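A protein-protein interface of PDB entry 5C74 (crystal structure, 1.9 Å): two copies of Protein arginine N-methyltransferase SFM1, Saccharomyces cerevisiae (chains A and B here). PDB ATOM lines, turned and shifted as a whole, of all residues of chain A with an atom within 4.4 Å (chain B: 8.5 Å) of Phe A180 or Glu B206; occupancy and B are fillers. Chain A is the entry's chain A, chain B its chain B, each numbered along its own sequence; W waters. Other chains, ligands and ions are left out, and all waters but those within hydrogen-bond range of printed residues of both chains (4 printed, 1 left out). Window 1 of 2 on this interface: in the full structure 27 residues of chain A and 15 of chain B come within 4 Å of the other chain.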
ATOM      1  N   TRP A  15       9.827  -1.554 -29.172  1.00  0.00           N
ATOM      2  CA  TRP A  15       9.692  -0.949 -27.847  1.00  0.00           C
ATOM      3  C   TRP A  15       9.794   0.573 -27.940  1.00  0.00           C
ATOM      4  O   TRP A  15       9.085   1.281 -27.213  1.00  0.00           O
ATOM      5  CB  TRP A  15      10.727  -1.506 -26.848  1.00  0.00           C
ATOM      6  CG  TRP A  15      12.185  -1.224 -27.131  1.00  0.00           C
ATOM      7  CD1 TRP A  15      13.072  -2.035 -27.787  1.00  0.00           C
ATOM      8  CD2 TRP A  15      12.928  -0.071 -26.720  1.00  0.00           C
ATOM      9  NE1 TRP A  15      14.318  -1.449 -27.816  1.00  0.00           N
ATOM     10  CE2 TRP A  15      14.257  -0.244 -27.161  1.00  0.00           C
ATOM     11  CE3 TRP A  15      12.595   1.102 -26.023  1.00  0.00           C
ATOM     12  CZ2 TRP A  15      15.255   0.703 -26.929  1.00  0.00           C
ATOM     13  CZ3 TRP A  15      13.593   2.044 -25.785  1.00  0.00           C
ATOM     14  CH2 TRP A  15      14.902   1.838 -26.245  1.00  0.00           C
ATOM     15  N   GLU A  19       7.078   3.359 -26.775  1.00  0.00           N
ATOM     16  CA  GLU A  19       7.436   4.495 -25.912  1.00  0.00           C
ATOM     17  C   GLU A  19       7.077   5.826 -26.541  1.00  0.00           C
ATOM     18  O   GLU A  19       6.483   6.689 -25.876  1.00  0.00           O
ATOM     19  CB  GLU A  19       8.921   4.467 -25.558  1.00  0.00           C
ATOM     20  CG  GLU A  19       9.241   3.286 -24.638  1.00  0.00           C
ATOM     21  CD  GLU A  19      10.573   3.409 -23.901  1.00  0.00           C
ATOM     22  OE1 GLU A  19      11.387   4.314 -24.227  1.00  0.00           O
ATOM     23  OE2 GLU A  19      10.784   2.589 -22.977  1.00  0.00           O
ATOM     24  N   GLN A 137      18.777   6.025 -14.102  1.00  0.00           N
ATOM     25  CA  GLN A 137      18.284   6.036 -15.477  1.00  0.00           C
ATOM     26  C   GLN A 137      16.794   5.728 -15.562  1.00  0.00           C
ATOM     27  O   GLN A 137      16.276   4.857 -14.842  1.00  0.00           O
ATOM     28  CB  GLN A 137      19.066   5.028 -16.332  1.00  0.00           C
ATOM     29  CG  GLN A 137      18.810   5.207 -17.828  1.00  0.00           C
ATOM     30  CD  GLN A 137      19.887   4.580 -18.691  1.00  0.00           C
ATOM     31  OE1 GLN A 137      20.219   3.402 -18.536  1.00  0.00           O
ATOM     32  NE2 GLN A 137      20.444   5.370 -19.607  1.00  0.00           N
ATOM     33  N   MET A 138      16.123   6.457 -16.448  1.00  0.00           N
ATOM     34  CA  MET A 138      14.712   6.283 -16.758  1.00  0.00           C
ATOM     35  C   MET A 138      14.536   5.990 -18.237  1.00  0.00           C
ATOM     36  O   MET A 138      15.346   6.448 -19.053  1.00  0.00           O
ATOM     37  CB  MET A 138      13.916   7.555 -16.421  1.00  0.00           C
ATOM     38  CG  MET A 138      14.011   8.030 -14.954  1.00  0.00           C
ATOM     39  SD  MET A 138      13.230   9.690 -14.759  1.00  0.00           S
ATOM     40  CE  MET A 138      12.879   9.584 -12.996  1.00  0.00           C
ATOM     41  N   THR A 139      13.465   5.284 -18.592  1.00  0.00           N
ATOM     42  CA  THR A 139      13.052   5.233 -19.986  1.00  0.00           C
ATOM     43  C   THR A 139      12.642   6.637 -20.418  1.00  0.00           C
ATOM     44  O   THR A 139      12.316   7.507 -19.596  1.00  0.00           O
ATOM     45  CB  THR A 139      11.875   4.252 -20.245  1.00  0.00           C
ATOM     46  OG1 THR A 139      10.693   4.714 -19.569  1.00  0.00           O
ATOM     47  CG2 THR A 139      12.227   2.818 -19.761  1.00  0.00           C
ATOM     48  N   ILE A 163       9.266   3.574  -8.444  1.00  0.00           N
ATOM     49  CA  ILE A 163       9.762   2.244  -8.109  1.00  0.00           C
ATOM     50  C   ILE A 163      11.039   2.034  -8.919  1.00  0.00           C
ATOM     51  O   ILE A 163      11.091   2.359 -10.100  1.00  0.00           O
ATOM     52  CB  ILE A 163       8.736   1.114  -8.402  1.00  0.00           C
ATOM     53  CG1 ILE A 163       9.306  -0.251  -7.995  1.00  0.00           C
ATOM     54  CG2 ILE A 163       8.296   1.092  -9.874  1.00  0.00           C
ATOM     55  CD1 ILE A 163       8.259  -1.347  -7.902  1.00  0.00           C
ATOM     56  N   ASP A 164      12.072   1.513  -8.276  1.00  0.00           N
ATOM     57  CA  ASP A 164      13.347   1.289  -8.941  1.00  0.00           C
ATOM     58  C   ASP A 164      13.493  -0.175  -9.313  1.00  0.00           C
ATOM     59  O   ASP A 164      13.304  -1.055  -8.467  1.00  0.00           O
ATOM     60  CB  ASP A 164      14.510   1.703  -8.032  1.00  0.00           C
ATOM     61  CG  ASP A 164      14.588   3.202  -7.826  1.00  0.00           C
ATOM     62  OD1 ASP A 164      14.014   3.955  -8.649  1.00  0.00           O
ATOM     63  OD2 ASP A 164      15.229   3.622  -6.837  1.00  0.00           O
ATOM     64  N   TYR A 165      13.854  -0.432 -10.565  1.00  0.00           N
ATOM     65  CA  TYR A 165      14.108  -1.786 -11.026  1.00  0.00           C
ATOM     66  C   TYR A 165      12.947  -2.746 -10.749  1.00  0.00           C
ATOM     67  O   TYR A 165      13.137  -3.784 -10.118  1.00  0.00           O
ATOM     68  CB  TYR A 165      15.386  -2.312 -10.377  1.00  0.00           C
ATOM     69  CG  TYR A 165      16.652  -1.828 -11.047  1.00  0.00           C
ATOM     70  CD1 TYR A 165      16.945  -0.472 -11.135  1.00  0.00           C
ATOM     71  CD2 TYR A 165      17.564  -2.731 -11.569  1.00  0.00           C
ATOM     72  CE1 TYR A 165      18.105  -0.029 -11.739  1.00  0.00           C
ATOM     73  CE2 TYR A 165      18.722  -2.296 -12.179  1.00  0.00           C
ATOM     74  CZ  TYR A 165      18.993  -0.947 -12.258  1.00  0.00           C
ATOM     75  OH  TYR A 165      20.158  -0.534 -12.867  1.00  0.00           O
ATOM     76  N   PRO A 166      11.740  -2.408 -11.230  1.00  0.00           N
ATOM     77  CA  PRO A 166      10.623  -3.322 -10.989  1.00  0.00           C
ATOM     78  C   PRO A 166      10.870  -4.669 -11.633  1.00  0.00           C
ATOM     79  O   PRO A 166      11.537  -4.746 -12.664  1.00  0.00           O
ATOM     80  CB  PRO A 166       9.451  -2.632 -11.664  1.00  0.00           C
ATOM     81  CG  PRO A 166      10.091  -1.819 -12.764  1.00  0.00           C
ATOM     82  CD  PRO A 166      11.357  -1.306 -12.125  1.00  0.00           C
ATOM     83  N   MET A 178      13.289  -4.832 -15.231  1.00  0.00           N
ATOM     84  CA  MET A 178      13.550  -3.642 -16.054  1.00  0.00           C
ATOM     85  C   MET A 178      14.379  -2.671 -15.227  1.00  0.00           C
ATOM     86  O   MET A 178      13.892  -2.120 -14.238  1.00  0.00           O
ATOM     87  CB  MET A 178      12.247  -2.971 -16.525  1.00  0.00           C
ATOM     88  CG  MET A 178      11.370  -3.871 -17.405  1.00  0.00           C
ATOM     89  SD  MET A 178      12.159  -4.588 -18.898  1.00  0.00           S
ATOM     90  CE  MET A 178      12.580  -3.110 -19.800  1.00  0.00           C
ATOM     91  N   PRO A 179      15.646  -2.472 -15.620  1.00  0.00           N
ATOM     92  CA  PRO A 179      16.623  -1.760 -14.796  1.00  0.00           C
ATOM     93  C   PRO A 179      16.504  -0.256 -14.901  1.00  0.00           C
ATOM     94  O   PRO A 179      17.476   0.404 -15.263  1.00  0.00           O
ATOM     95  CB  PRO A 179      17.964  -2.236 -15.373  1.00  0.00           C
ATOM     96  CG  PRO A 179      17.651  -2.484 -16.820  1.00  0.00           C
ATOM     97  CD  PRO A 179      16.274  -3.089 -16.810  1.00  0.00           C
ATOM     98  N   PHE A 180      15.323   0.265 -14.578  1.00  0.00           N
ATOM     99  CA  PHE A 180      15.036   1.685 -14.676  1.00  0.00           C
ATOM    100  C   PHE A 180      14.218   2.109 -13.489  1.00  0.00           C
ATOM    101  O   PHE A 180      13.629   1.279 -12.798  1.00  0.00           O
ATOM    102  CB  PHE A 180      14.269   2.007 -15.962  1.00  0.00           C
ATOM    103  CG  PHE A 180      14.993   1.594 -17.195  1.00  0.00           C
ATOM    104  CD1 PHE A 180      15.959   2.423 -17.748  1.00  0.00           C
ATOM    105  CD2 PHE A 180      14.727   0.376 -17.791  1.00  0.00           C
ATOM    106  CE1 PHE A 180      16.657   2.032 -18.892  1.00  0.00           C
ATOM    107  CE2 PHE A 180      15.420  -0.017 -18.924  1.00  0.00           C
ATOM    108  CZ  PHE A 180      16.385   0.813 -19.472  1.00  0.00           C
ATOM    109  N   ARG A 181      14.174   3.415 -13.275  1.00  0.00           N
ATOM    110  CA  ARG A 181      13.292   3.989 -12.292  1.00  0.00           C
ATOM    111  C   ARG A 181      12.004   4.359 -13.014  1.00  0.00           C
ATOM    112  O   ARG A 181      12.058   5.031 -14.048  1.00  0.00           O
ATOM    113  CB  ARG A 181      13.946   5.217 -11.653  1.00  0.00           C
ATOM    114  CG  ARG A 181      12.997   6.084 -10.840  1.00  0.00           C
ATOM    115  CD  ARG A 181      13.792   7.163 -10.091  1.00  0.00           C
ATOM    116  NE  ARG A 181      14.529   6.590  -8.969  1.00  0.00           N
ATOM    117  CZ  ARG A 181      15.518   7.197  -8.314  1.00  0.00           C
ATOM    118  NH1 ARG A 181      15.938   8.409  -8.678  1.00  0.00           N
ATOM    119  NH2 ARG A 181      16.101   6.571  -7.295  1.00  0.00           N
ATOM    120  N   TYR A 182      10.862   3.909 -12.487  1.00  0.00           N
ATOM    121  CA  TYR A 182       9.561   4.200 -13.100  1.00  0.00           C
ATOM    122  C   TYR A 182       8.663   5.002 -12.163  1.00  0.00           C
ATOM    123  O   TYR A 182       8.768   4.885 -10.944  1.00  0.00           O
ATOM    124  CB  TYR A 182       8.828   2.912 -13.482  1.00  0.00           C
ATOM    125  CG  TYR A 182       9.454   2.115 -14.603  1.00  0.00           C
ATOM    126  CD1 TYR A 182      10.481   1.215 -14.344  1.00  0.00           C
ATOM    127  CD2 TYR A 182       9.006   2.241 -15.916  1.00  0.00           C
ATOM    128  CE1 TYR A 182      11.057   0.459 -15.368  1.00  0.00           C
ATOM    129  CE2 TYR A 182       9.574   1.485 -16.948  1.00  0.00           C
ATOM    130  CZ  TYR A 182      10.598   0.601 -16.662  1.00  0.00           C
ATOM    131  OH  TYR A 182      11.168  -0.152 -17.673  1.00  0.00           O
ATOM    132  N   ASN B 171      23.510  -1.162 -29.109  1.00  0.00           N
ATOM    133  CA  ASN B 171      23.597  -0.026 -28.210  1.00  0.00           C
ATOM    134  C   ASN B 171      22.651  -0.225 -27.026  1.00  0.00           C
ATOM    135  O   ASN B 171      21.816  -1.130 -27.044  1.00  0.00           O
ATOM    136  CB  ASN B 171      23.265   1.262 -28.966  1.00  0.00           C
ATOM    137  CG  ASN B 171      23.999   2.471 -28.419  1.00  0.00           C
ATOM    138  OD1 ASN B 171      24.853   2.350 -27.539  1.00  0.00           O
ATOM    139  ND2 ASN B 171      23.674   3.648 -28.948  1.00  0.00           N
ATOM    140  N   LYS B 172      22.792   0.610 -26.000  1.00  0.00           N
ATOM    141  CA  LYS B 172      21.842   0.630 -24.884  1.00  0.00           C
ATOM    142  C   LYS B 172      21.675  -0.735 -24.209  1.00  0.00           C
ATOM    143  O   LYS B 172      20.566  -1.103 -23.807  1.00  0.00           O
ATOM    144  CB  LYS B 172      20.479   1.132 -25.369  1.00  0.00           C
ATOM    145  CG  LYS B 172      20.517   2.500 -26.053  1.00  0.00           C
ATOM    146  CD  LYS B 172      19.131   2.956 -26.503  1.00  0.00           C
ATOM    147  CE  LYS B 172      19.192   4.350 -27.139  1.00  0.00           C
ATOM    148  NZ  LYS B 172      17.848   4.936 -27.404  1.00  0.00           N
ATOM    149  N   ASN B 173      22.775  -1.480 -24.116  1.00  0.00           N
ATOM    150  CA  ASN B 173      22.806  -2.781 -23.447  1.00  0.00           C
ATOM    151  C   ASN B 173      21.806  -3.812 -23.971  1.00  0.00           C
ATOM    152  O   ASN B 173      21.247  -4.589 -23.205  1.00  0.00           O
ATOM    153  CB  ASN B 173      22.600  -2.598 -21.942  1.00  0.00           C
ATOM    154  CG  ASN B 173      23.789  -1.950 -21.273  1.00  0.00           C
ATOM    155  OD1 ASN B 173      24.793  -2.608 -20.996  1.00  0.00           O
ATOM    156  ND2 ASN B 173      23.690  -0.649 -21.023  1.00  0.00           N
ATOM    157  N   GLU B 174      21.602  -3.849 -25.282  1.00  0.00           N
ATOM    158  CA  GLU B 174      20.781  -4.907 -25.847  1.00  0.00           C
ATOM    159  C   GLU B 174      21.634  -5.968 -26.516  1.00  0.00           C
ATOM    160  O   GLU B 174      22.756  -5.696 -26.949  1.00  0.00           O
ATOM    161  CB  GLU B 174      19.780  -4.333 -26.831  1.00  0.00           C
ATOM    162  CG  GLU B 174      18.845  -3.349 -26.186  1.00  0.00           C
ATOM    163  CD  GLU B 174      17.958  -2.682 -27.191  1.00  0.00           C
ATOM    164  OE1 GLU B 174      17.596  -1.510 -26.968  1.00  0.00           O
ATOM    165  OE2 GLU B 174      17.628  -3.332 -28.211  1.00  0.00           O
ATOM    166  N   ALA B 175      21.103  -7.182 -26.572  1.00  0.00           N
ATOM    167  CA  ALA B 175      21.776  -8.281 -27.244  1.00  0.00           C
ATOM    168  C   ALA B 175      20.750  -9.311 -27.682  1.00  0.00           C
ATOM    169  O   ALA B 175      19.711  -9.472 -27.044  1.00  0.00           O
ATOM    170  CB  ALA B 175      22.832  -8.919 -26.340  1.00  0.00           C
ATOM    171  N   LYS B 201      17.637  -5.844 -34.636  1.00  0.00           N
ATOM    172  CA  LYS B 201      17.569  -4.788 -33.623  1.00  0.00           C
ATOM    173  C   LYS B 201      16.120  -4.356 -33.376  1.00  0.00           C
ATOM    174  O   LYS B 201      15.726  -4.069 -32.248  1.00  0.00           O
ATOM    175  CB  LYS B 201      18.425  -3.595 -34.063  1.00  0.00           C
ATOM    176  CG  LYS B 201      18.567  -2.493 -33.027  1.00  0.00           C
ATOM    177  CD  LYS B 201      19.530  -1.414 -33.507  1.00  0.00           C
ATOM    178  CE  LYS B 201      19.527  -0.210 -32.569  1.00  0.00           C
ATOM    179  NZ  LYS B 201      19.915  -0.598 -31.181  1.00  0.00           N
ATOM    180  N   LYS B 202      15.322  -4.349 -34.437  1.00  0.00           N
ATOM    181  CA  LYS B 202      13.952  -3.855 -34.359  1.00  0.00           C
ATOM    182  C   LYS B 202      13.104  -4.706 -33.420  1.00  0.00           C
ATOM    183  O   LYS B 202      12.198  -4.193 -32.756  1.00  0.00           O
ATOM    184  CB  LYS B 202      13.330  -3.811 -35.757  1.00  0.00           C
ATOM    185  CG  LYS B 202      11.923  -3.220 -35.842  1.00  0.00           C
ATOM    186  CD  LYS B 202      11.512  -3.052 -37.315  1.00  0.00           C
ATOM    187  CE  LYS B 202      10.113  -2.457 -37.468  1.00  0.00           C
ATOM    188  NZ  LYS B 202       9.992  -1.072 -36.910  1.00  0.00           N
ATOM    189  N   ASP B 203      13.406  -6.001 -33.347  1.00  0.00           N
ATOM    190  CA  ASP B 203      12.646  -6.906 -32.489  1.00  0.00           C
ATOM    191  C   ASP B 203      13.338  -7.208 -31.158  1.00  0.00           C
ATOM    192  O   ASP B 203      12.838  -8.011 -30.373  1.00  0.00           O
ATOM    193  CB  ASP B 203      12.362  -8.227 -33.215  1.00  0.00           C
ATOM    194  CG  ASP B 203      11.103  -8.174 -34.055  1.00  0.00           C
ATOM    195  OD1 ASP B 203      10.194  -7.380 -33.710  1.00  0.00           O
ATOM    196  OD2 ASP B 203      11.022  -8.935 -35.048  1.00  0.00           O
ATOM    197  N   SER B 204      14.484  -6.578 -30.912  1.00  0.00           N
ATOM    198  CA  SER B 204      15.179  -6.747 -29.641  1.00  0.00           C
ATOM    199  C   SER B 204      14.554  -5.880 -28.555  1.00  0.00           C
ATOM    200  O   SER B 204      14.399  -4.688 -28.744  1.00  0.00           O
ATOM    201  CB  SER B 204      16.658  -6.396 -29.783  1.00  0.00           C
ATOM    202  OG  SER B 204      17.274  -7.213 -30.763  1.00  0.00           O
ATOM    203  N   LEU B 205      14.231  -6.473 -27.409  1.00  0.00           N
ATOM    204  CA  LEU B 205      13.614  -5.710 -26.326  1.00  0.00           C
ATOM    205  C   LEU B 205      14.630  -4.799 -25.638  1.00  0.00           C
ATOM    206  O   LEU B 205      15.812  -5.146 -25.528  1.00  0.00           O
ATOM    207  CB  LEU B 205      12.978  -6.656 -25.298  1.00  0.00           C
ATOM    208  CG  LEU B 205      12.239  -6.037 -24.104  1.00  0.00           C
ATOM    209  CD1 LEU B 205      10.981  -5.297 -24.536  1.00  0.00           C
ATOM    210  CD2 LEU B 205      11.899  -7.116 -23.073  1.00  0.00           C
ATOM    211  N   GLU B 206      14.156  -3.642 -25.175  1.00  0.00           N
ATOM    212  CA  GLU B 206      14.931  -2.724 -24.331  1.00  0.00           C
ATOM    213  C   GLU B 206      15.700  -3.450 -23.220  1.00  0.00           C
ATOM    214  O   GLU B 206      15.232  -4.466 -22.684  1.00  0.00           O
ATOM    215  CB  GLU B 206      13.983  -1.684 -23.706  1.00  0.00           C
ATOM    216  CG  GLU B 206      14.659  -0.626 -22.866  1.00  0.00           C
ATOM    217  CD  GLU B 206      13.783   0.604 -22.627  1.00  0.00           C
ATOM    218  OE1 GLU B 206      14.348   1.702 -22.441  1.00  0.00           O
ATOM    219  OE2 GLU B 206      12.544   0.477 -22.614  1.00  0.00           O
ATOM    220  N   HIS B 207      16.885  -2.948 -22.905  1.00  0.00           N
ATOM    221  CA  HIS B 207      17.679  -3.414 -21.769  1.00  0.00           C
ATOM    222  C   HIS B 207      16.879  -3.997 -20.616  1.00  0.00           C
ATOM    223  O   HIS B 207      16.071  -3.316 -20.016  1.00  0.00           O
ATOM    224  CB  HIS B 207      18.552  -2.222 -21.354  1.00  0.00           C
ATOM    225  CG  HIS B 207      19.532  -2.487 -20.251  1.00  0.00           C
ATOM    226  ND1 HIS B 207      19.713  -1.596 -19.227  1.00  0.00           N
ATOM    227  CD2 HIS B 207      20.164  -3.621 -19.870  1.00  0.00           C
ATOM    228  CE1 HIS B 207      20.595  -2.090 -18.368  1.00  0.00           C
ATOM    229  NE2 HIS B 207      20.862  -3.335 -18.727  1.00  0.00           N
ATOM    230  N   HIS B 208      17.084  -5.291 -20.362  1.00  0.00           N
ATOM    231  CA  HIS B 208      16.302  -6.010 -19.357  1.00  0.00           C
ATOM    232  C   HIS B 208      17.095  -7.186 -18.822  1.00  0.00           C
ATOM    233  O   HIS B 208      18.046  -7.631 -19.464  1.00  0.00           O
ATOM    234  CB  HIS B 208      14.974  -6.501 -19.950  1.00  0.00           C
ATOM    235  CG  HIS B 208      15.139  -7.524 -21.040  1.00  0.00           C
ATOM    236  ND1 HIS B 208      15.543  -7.195 -22.315  1.00  0.00           N
ATOM    237  CD2 HIS B 208      14.967  -8.869 -21.035  1.00  0.00           C
ATOM    238  CE1 HIS B 208      15.603  -8.290 -23.056  1.00  0.00           C
ATOM    239  NE2 HIS B 208      15.257  -9.321 -22.303  1.00  0.00           N
ATOM    240  N   HIS B 209      16.695  -7.709 -17.664  1.00  0.00           N
ATOM    241  CA  HIS B 209      17.404  -8.835 -17.065  1.00  0.00           C
ATOM    242  C   HIS B 209      16.465 -10.001 -16.795  1.00  0.00           C
ATOM    243  O   HIS B 209      15.392  -9.833 -16.208  1.00  0.00           O
ATOM    244  CB  HIS B 209      18.076  -8.431 -15.743  1.00  0.00           C
ATOM    245  CG  HIS B 209      18.996  -7.252 -15.849  1.00  0.00           C
ATOM    246  ND1 HIS B 209      19.011  -6.240 -14.915  1.00  0.00           N
ATOM    247  CD2 HIS B 209      19.977  -6.956 -16.738  1.00  0.00           C
ATOM    248  CE1 HIS B 209      19.923  -5.341 -15.252  1.00  0.00           C
ATOM    249  NE2 HIS B 209      20.532  -5.761 -16.348  1.00  0.00           N
ATOM    250  N   HIS B 210      16.879 -11.194 -17.189  1.00  0.00           N
ATOM    251  CA  HIS B 210      16.049 -12.362 -16.951  1.00  0.00           C
ATOM    252  C   HIS B 210      16.309 -12.943 -15.572  1.00  0.00           C
ATOM    253  O   HIS B 210      17.434 -13.346 -15.247  1.00  0.00           O
ATOM    254  CB  HIS B 210      16.277 -13.408 -18.045  1.00  0.00           C
ATOM    255  CG  HIS B 210      15.672 -13.023 -19.358  1.00  0.00           C
ATOM    256  ND1 HIS B 210      14.336 -13.206 -19.635  1.00  0.00           N
ATOM    257  CD2 HIS B 210      16.207 -12.432 -20.452  1.00  0.00           C
ATOM    258  CE1 HIS B 210      14.073 -12.757 -20.852  1.00  0.00           C
ATOM    259  NE2 HIS B 210      15.193 -12.289 -21.374  1.00  0.00           N
HETATM  260  O   HOH W   1      13.910   4.492 -23.274  1.00  0.00           O
HETATM  261  O   HOH W   2      11.417  -4.263 -29.762  1.00  0.00           O
HETATM  262  O   HOH W   3      19.980   1.188 -20.320  1.00  0.00           O
HETATM  263  O   HOH W   4      19.372   0.912 -17.357  1.00  0.00           O
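Of chain B, only Glu B206 and His B207 come within 4 Å of Phe A180.
Of chain A, only Trp A15, Glu A19, Thr A139 and Phe A180 come within 4 Å of Glu B206.
Of the printed residues of chain B, Glu A19 touches Glu B206.
Of the printed residues of chain B, Met A178 touches His B207 and His B208.
Lys B201 touches none of the printed residues of chain A.
The nearest residue of chain B that does not touch Phe A180 is His B208 (5.7 Å).
The nearest residue of chain A that does not touch Glu B206 is Met A178 (4.1 Å).
The nearest printed residue of chain A that does not touch His B207 is Gln A137 (5.1 Å).
Among the printed residues, merely in contact across the chains: Trp A15 with Leu B205, Thr A139 with Glu B206, Met A178 with His B207, Met A178 with His B208, Pro A179 with His B207, Pro A179 with His B208, Pro A179 with His B209, Phe A180 with Glu B206 and Phe A180 with His B207.
Water W1 bridges the side-chain carboxylate of Glu A19 (2.7 Å) and the side-chain carboxylate of Glu B206 (2.9 Å).
Water W3 lies within hydrogen-bond range of the side-chain amide oxygen of Gln A137 (2.9 Å) and a ring nitrogen (ND1) of His B207 (3.0 Å).
Water W4 lies within hydrogen-bond range of the backbone carbonyl oxygen (O) of Pro A179, the side-chain amide oxygen (OE1) of Gln A137 and a ring nitrogen (ND1) of His B207.
Water W2 lies within hydrogen-bond range of O of Lys B202 (3.1 Å), O of Ser B204 (3.2 Å) and N of Trp A15 (3.2 Å).
Among the printed residues, 13 pairs touch across the chains.
The side-chain carboxylate (OE1) of Glu B174 lies close to the indole nitrogen (NE1) of Trp A15 (3.4 Å).
The indole nitrogen of Trp A15 lies close to the backbone carbonyl oxygen of Ser B204 (3.4 Å).
The indole nitrogen (NE1) of Trp A15 sits close to the backbone NH (N) of Glu B206 (3.4 Å).
The side-chain carboxylate of Glu A19 lies close to the side-chain carboxylate of Glu B206, at 2.8 Å.
N of Tyr A165 sits at hydrogen-bond distance from O of Phe A180.
The backbone carbonyl oxygen of Pro A166 sits at hydrogen-bond distance from the backbone NH of Met A178 (3.1 Å).
O of Glu B206 is in hydrogen-bond range of ND1 of His B208 (2.8 Å).
A ring nitrogen (NE2) of His B207 lies within hydrogen-bond range of a ring nitrogen (NE2) of His B209 (3.4 Å).
No position is printed for both chains.
Of the 13 pairs that touch across the chains among the printed residues, none has its exchanged pair printed and touching as well.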
